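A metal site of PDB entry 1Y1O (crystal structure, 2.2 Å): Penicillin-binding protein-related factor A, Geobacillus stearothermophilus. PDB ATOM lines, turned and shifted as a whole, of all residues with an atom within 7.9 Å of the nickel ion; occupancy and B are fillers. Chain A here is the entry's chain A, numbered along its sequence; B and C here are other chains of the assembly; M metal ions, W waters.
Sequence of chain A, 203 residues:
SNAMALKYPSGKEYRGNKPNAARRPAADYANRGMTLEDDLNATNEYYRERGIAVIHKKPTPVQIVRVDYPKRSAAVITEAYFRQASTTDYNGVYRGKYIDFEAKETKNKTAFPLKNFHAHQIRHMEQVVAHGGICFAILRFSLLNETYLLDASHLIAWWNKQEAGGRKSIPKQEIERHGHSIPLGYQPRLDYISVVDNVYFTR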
ATOM      1  N   LEU A 150      -3.939   6.177  19.752  1.00  0.00           N
ATOM      2  CA  LEU A 150      -4.612   7.450  20.087  1.00  0.00           C
ATOM      3  C   LEU A 150      -5.691   7.724  19.042  1.00  0.00           C
ATOM      4  O   LEU A 150      -5.388   7.854  17.861  1.00  0.00           O
ATOM      5  CB  LEU A 150      -3.609   8.620  20.120  1.00  0.00           C
ATOM      6  CG  LEU A 150      -4.109   9.967  20.660  1.00  0.00           C
ATOM      7  CD1 LEU A 150      -4.531   9.854  22.142  1.00  0.00           C
ATOM      8  CD2 LEU A 150      -3.046  11.089  20.449  1.00  0.00           C
ATOM      9  N   ASP A 151      -6.947   7.795  19.480  1.00  0.00           N
ATOM     10  CA  ASP A 151      -8.029   8.163  18.593  1.00  0.00           C
ATOM     11  C   ASP A 151      -7.739   9.471  17.829  1.00  0.00           C
ATOM     12  O   ASP A 151      -7.113  10.387  18.355  1.00  0.00           O
ATOM     13  CB  ASP A 151      -9.327   8.260  19.391  1.00  0.00           C
ATOM     14  CG  ASP A 151     -10.504   8.566  18.514  1.00  0.00           C
ATOM     15  OD1 ASP A 151     -10.847   7.702  17.706  1.00  0.00           O
ATOM     16  OD2 ASP A 151     -11.084   9.675  18.626  1.00  0.00           O
ATOM     17  N   SER A 153      -9.417  11.974  17.104  1.00  0.00           N
ATOM     18  CA  SER A 153      -9.985  13.179  17.697  1.00  0.00           C
ATOM     19  C   SER A 153      -9.009  13.983  18.513  1.00  0.00           C
ATOM     20  O   SER A 153      -8.992  15.204  18.429  1.00  0.00           O
ATOM     21  CB  SER A 153     -11.241  12.820  18.528  1.00  0.00           C
ATOM     22  OG  SER A 153     -10.822  12.046  19.632  1.00  0.00           O
ATOM     23  N   HIS A 154      -8.154  13.276  19.281  1.00  0.00           N
ATOM     24  CA  HIS A 154      -7.070  13.863  20.031  1.00  0.00           C
ATOM     25  C   HIS A 154      -5.970  14.409  19.125  1.00  0.00           C
ATOM     26  O   HIS A 154      -5.458  15.495  19.380  1.00  0.00           O
ATOM     27  CB  HIS A 154      -6.492  12.839  21.024  1.00  0.00           C
ATOM     28  CG  HIS A 154      -7.541  12.252  21.920  1.00  0.00           C
ATOM     29  ND1 HIS A 154      -7.965  12.868  23.081  1.00  0.00           N
ATOM     30  CD2 HIS A 154      -8.269  11.125  21.797  1.00  0.00           C
ATOM     31  CE1 HIS A 154      -8.916  12.141  23.635  1.00  0.00           C
ATOM     32  NE2 HIS A 154      -9.133  11.092  22.871  1.00  0.00           N
ATOM     33  N   LEU A 155      -5.609  13.677  18.068  1.00  0.00           N
ATOM     34  CA  LEU A 155      -4.514  14.115  17.215  1.00  0.00           C
ATOM     35  C   LEU A 155      -4.962  15.364  16.456  1.00  0.00           C
ATOM     36  O   LEU A 155      -4.184  16.309  16.323  1.00  0.00           O
ATOM     37  CB  LEU A 155      -4.145  13.005  16.219  1.00  0.00           C
ATOM     38  CG  LEU A 155      -3.013  13.227  15.250  1.00  0.00           C
ATOM     39  CD1 LEU A 155      -1.738  13.778  15.984  1.00  0.00           C
ATOM     40  CD2 LEU A 155      -2.718  11.884  14.503  1.00  0.00           C
ATOM     41  N   ALA A 157      -7.258  17.601  17.472  1.00  0.00           N
ATOM     42  CA  ALA A 157      -7.294  18.770  18.390  1.00  0.00           C
ATOM     43  C   ALA A 157      -5.875  19.342  18.657  1.00  0.00           C
ATOM     44  O   ALA A 157      -5.631  20.557  18.518  1.00  0.00           O
ATOM     45  CB  ALA A 157      -8.027  18.427  19.726  1.00  0.00           C
ATOM     46  N   TRP A 158      -4.940  18.455  19.008  1.00  0.00           N
ATOM     47  CA  TRP A 158      -3.537  18.882  19.183  1.00  0.00           C
ATOM     48  C   TRP A 158      -2.874  19.503  17.933  1.00  0.00           C
ATOM     49  O   TRP A 158      -2.212  20.548  17.983  1.00  0.00           O
ATOM     50  CB  TRP A 158      -2.702  17.712  19.714  1.00  0.00           C
ATOM     51  CG  TRP A 158      -2.939  17.552  21.171  1.00  0.00           C
ATOM     52  CD1 TRP A 158      -3.924  16.819  21.757  1.00  0.00           C
ATOM     53  CD2 TRP A 158      -2.221  18.200  22.233  1.00  0.00           C
ATOM     54  NE1 TRP A 158      -3.858  16.958  23.120  1.00  0.00           N
ATOM     55  CE2 TRP A 158      -2.817  17.797  23.446  1.00  0.00           C
ATOM     56  CE3 TRP A 158      -1.128  19.071  22.281  1.00  0.00           C
ATOM     57  CZ2 TRP A 158      -2.327  18.201  24.705  1.00  0.00           C
ATOM     58  CZ3 TRP A 158      -0.650  19.508  23.532  1.00  0.00           C
ATOM     59  CH2 TRP A 158      -1.268  19.081  24.728  1.00  0.00           C
ATOM     60  N   ILE A 170       2.830  16.593  21.300  1.00  0.00           N
ATOM     61  CA  ILE A 170       1.894  16.078  22.274  1.00  0.00           C
ATOM     62  C   ILE A 170       2.655  15.552  23.478  1.00  0.00           C
ATOM     63  O   ILE A 170       3.417  14.617  23.340  1.00  0.00           O
ATOM     64  CB  ILE A 170       1.020  14.960  21.694  1.00  0.00           C
ATOM     65  CG1 ILE A 170       0.369  15.407  20.386  1.00  0.00           C
ATOM     66  CG2 ILE A 170      -0.010  14.552  22.726  1.00  0.00           C
ATOM     67  CD1 ILE A 170      -0.378  14.369  19.652  1.00  0.00           C
ATOM     68  N   GLU A 174      -0.511  13.316  27.994  1.00  0.00           N
ATOM     69  CA  GLU A 174      -1.735  13.343  27.204  1.00  0.00           C
ATOM     70  C   GLU A 174      -1.999  11.993  26.504  1.00  0.00           C
ATOM     71  O   GLU A 174      -3.110  11.453  26.563  1.00  0.00           O
ATOM     72  CB  GLU A 174      -1.669  14.479  26.169  1.00  0.00           C
ATOM     73  CG  GLU A 174      -2.428  14.209  24.872  1.00  0.00           C
ATOM     74  CD  GLU A 174      -3.964  14.275  25.017  1.00  0.00           C
ATOM     75  OE1 GLU A 174      -4.459  14.972  25.952  1.00  0.00           O
ATOM     76  OE2 GLU A 174      -4.661  13.647  24.178  1.00  0.00           O
ATOM     77  N   ILE A 175      -0.951  11.452  25.888  1.00  0.00           N
ATOM     78  CA  ILE A 175      -0.996  10.139  25.235  1.00  0.00           C
ATOM     79  C   ILE A 175      -1.283   9.042  26.254  1.00  0.00           C
ATOM     80  O   ILE A 175      -2.100   8.167  26.000  1.00  0.00           O
ATOM     81  CB  ILE A 175       0.343   9.836  24.443  1.00  0.00           C
ATOM     82  CG1 ILE A 175       0.540  10.887  23.334  1.00  0.00           C
ATOM     83  CG2 ILE A 175       0.331   8.386  23.902  1.00  0.00           C
ATOM     84  CD1 ILE A 175       1.865  10.879  22.642  1.00  0.00           C
ATOM     85  N   ARG A 177      -2.828   9.614  29.237  1.00  0.00           N
ATOM     86  CA  ARG A 177      -4.180   9.898  29.735  1.00  0.00           C
ATOM     87  C   ARG A 177      -5.317   9.508  28.750  1.00  0.00           C
ATOM     88  O   ARG A 177      -6.317   8.919  29.139  1.00  0.00           O
ATOM     89  CB  ARG A 177      -4.270  11.396  30.053  1.00  0.00           C
ATOM     90  CG  ARG A 177      -5.140  11.713  31.250  1.00  0.00           C
ATOM     91  CD  ARG A 177      -5.051  13.169  31.578  1.00  0.00           C
ATOM     92  NE  ARG A 177      -3.860  13.434  32.359  1.00  0.00           N
ATOM     93  CZ  ARG A 177      -2.833  14.195  31.970  1.00  0.00           C
ATOM     94  NH1 ARG A 177      -2.815  14.804  30.787  1.00  0.00           N
ATOM     95  NH2 ARG A 177      -1.822  14.332  32.793  1.00  0.00           N
ATOM     96  N   HIS A 178      -5.179   9.874  27.487  1.00  0.00           N
ATOM     97  CA  HIS A 178      -6.279   9.668  26.554  1.00  0.00           C
ATOM     98  C   HIS A 178      -6.005   8.557  25.541  1.00  0.00           C
ATOM     99  O   HIS A 178      -6.895   8.180  24.810  1.00  0.00           O
ATOM    100  CB  HIS A 178      -6.536  10.957  25.781  1.00  0.00           C
ATOM    101  CG  HIS A 178      -7.121  12.060  26.604  1.00  0.00           C
ATOM    102  ND1 HIS A 178      -7.159  13.360  26.161  1.00  0.00           N
ATOM    103  CD2 HIS A 178      -7.701  12.061  27.830  1.00  0.00           C
ATOM    104  CE1 HIS A 178      -7.741  14.113  27.074  1.00  0.00           C
ATOM    105  NE2 HIS A 178      -8.069  13.351  28.098  1.00  0.00           N
ATOM    106  N   GLY A 179      -4.775   8.045  25.479  1.00  0.00           N
ATOM    107  CA  GLY A 179      -4.455   6.947  24.578  1.00  0.00           C
ATOM    108  C   GLY A 179      -4.417   5.613  25.341  1.00  0.00           C
ATOM    109  O   GLY A 179      -4.772   5.538  26.489  1.00  0.00           O
ATOM    110  N   GLU B 126     -13.304  20.939  18.378  1.00  0.00           N
ATOM    111  CA  GLU B 126     -12.343  19.796  18.298  1.00  0.00           C
ATOM    112  C   GLU B 126     -11.998  19.278  19.678  1.00  0.00           C
ATOM    113  O   GLU B 126     -11.912  18.086  19.902  1.00  0.00           O
ATOM    114  CB  GLU B 126     -11.059  20.214  17.570  1.00  0.00           C
ATOM    115  CG  GLU B 126     -11.250  20.526  16.065  1.00  0.00           C
ATOM    116  CD  GLU B 126     -10.102  21.371  15.457  1.00  0.00           C
ATOM    117  OE1 GLU B 126      -9.213  21.840  16.247  1.00  0.00           O
ATOM    118  OE2 GLU B 126     -10.067  21.565  14.200  1.00  0.00           O
ATOM    119  N   GLN B 127     -11.763  20.214  20.597  1.00  0.00           N
ATOM    120  CA  GLN B 127     -11.391  19.892  21.986  1.00  0.00           C
ATOM    121  C   GLN B 127     -12.550  19.242  22.741  1.00  0.00           C
ATOM    122  O   GLN B 127     -12.324  18.338  23.536  1.00  0.00           O
ATOM    123  CB  GLN B 127     -10.926  21.164  22.726  1.00  0.00           C
ATOM    124  CG  GLN B 127      -9.477  21.534  22.428  1.00  0.00           C
ATOM    125  CD  GLN B 127      -9.197  22.992  22.705  1.00  0.00           C
ATOM    126  OE1 GLN B 127      -9.306  23.454  23.859  1.00  0.00           O
ATOM    127  NE2 GLN B 127      -8.820  23.750  21.650  1.00  0.00           N
ATOM    128  N   ALA B 130     -12.843  15.761  21.452  1.00  0.00           N
ATOM    129  CA  ALA B 130     -11.760  14.923  22.033  1.00  0.00           C
ATOM    130  C   ALA B 130     -12.001  14.533  23.512  1.00  0.00           C
ATOM    131  O   ALA B 130     -11.584  13.449  23.959  1.00  0.00           O
ATOM    132  CB  ALA B 130     -10.399  15.556  21.840  1.00  0.00           C
ATOM    133  N   HIS B 131     -12.760  15.371  24.245  1.00  0.00           N
ATOM    134  CA  HIS B 131     -13.072  15.141  25.671  1.00  0.00           C
ATOM    135  C   HIS B 131     -14.403  14.468  25.930  1.00  0.00           C
ATOM    136  O   HIS B 131     -14.842  14.335  27.075  1.00  0.00           O
ATOM    137  CB  HIS B 131     -12.983  16.467  26.451  1.00  0.00           C
ATOM    138  CG  HIS B 131     -11.579  16.895  26.711  1.00  0.00           C
ATOM    139  ND1 HIS B 131     -10.829  17.610  25.779  1.00  0.00           N
ATOM    140  CD2 HIS B 131     -10.770  16.709  27.787  1.00  0.00           C
ATOM    141  CE1 HIS B 131      -9.628  17.852  26.283  1.00  0.00           C
ATOM    142  NE2 HIS B 131      -9.564  17.323  27.506  1.00  0.00           N
ATOM    143  N   ARG C  50      -2.692  21.308  28.738  1.00  0.00           N
ATOM    144  CA  ARG C  50      -2.263  19.935  28.894  1.00  0.00           C
ATOM    145  C   ARG C  50      -3.295  18.890  28.385  1.00  0.00           C
ATOM    146  O   ARG C  50      -3.046  17.694  28.434  1.00  0.00           O
ATOM    147  CB  ARG C  50      -1.917  19.678  30.367  1.00  0.00           C
ATOM    148  CG  ARG C  50      -0.837  20.606  30.977  1.00  0.00           C
ATOM    149  CD  ARG C  50       0.534  20.381  30.376  1.00  0.00           C
ATOM    150  NE  ARG C  50       1.087  19.069  30.753  1.00  0.00           N
ATOM    151  CZ  ARG C  50       2.280  18.614  30.347  1.00  0.00           C
ATOM    152  NH1 ARG C  50       3.047  19.353  29.560  1.00  0.00           N
ATOM    153  NH2 ARG C  50       2.714  17.422  30.758  1.00  0.00           N
ATOM    154  N   GLY C  51      -4.454  19.355  27.905  1.00  0.00           N
ATOM    155  CA  GLY C  51      -5.529  18.470  27.475  1.00  0.00           C
ATOM    156  C   GLY C  51      -6.189  17.688  28.613  1.00  0.00           C
ATOM    157  O   GLY C  51      -6.681  16.596  28.402  1.00  0.00           O
ATOM    158  N   ILE C  52      -6.177  18.239  29.818  1.00  0.00           N
ATOM    159  CA  ILE C  52      -6.721  17.543  30.964  1.00  0.00           C
ATOM    160  C   ILE C  52      -8.243  17.737  31.100  1.00  0.00           C
ATOM    161  O   ILE C  52      -8.972  16.784  31.394  1.00  0.00           O
ATOM    162  CB  ILE C  52      -6.010  17.978  32.275  1.00  0.00           C
ATOM    163  CG1 ILE C  52      -4.551  17.446  32.287  1.00  0.00           C
ATOM    164  CG2 ILE C  52      -6.779  17.442  33.480  1.00  0.00           C
ATOM    165  CD1 ILE C  52      -3.769  17.802  33.546  1.00  0.00           C
HETATM  166 NI    NI M   1      -6.750  14.081  24.218  1.00  0.00          NI
HETATM  167  O   HOH W   1      -7.167  16.211  23.709  1.00  0.00           O
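Within 4 Å of the nickel ion: His 154, Glu 174 and His 178.
The nickel ion is bound by a ring nitrogen (ND1) of His 154 (2.1 Å), a ring nitrogen (ND1) of His 178 (2.1 Å), the side-chain carboxylate of Glu 174 (2.1 Å) and water W1 (2.2 Å).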
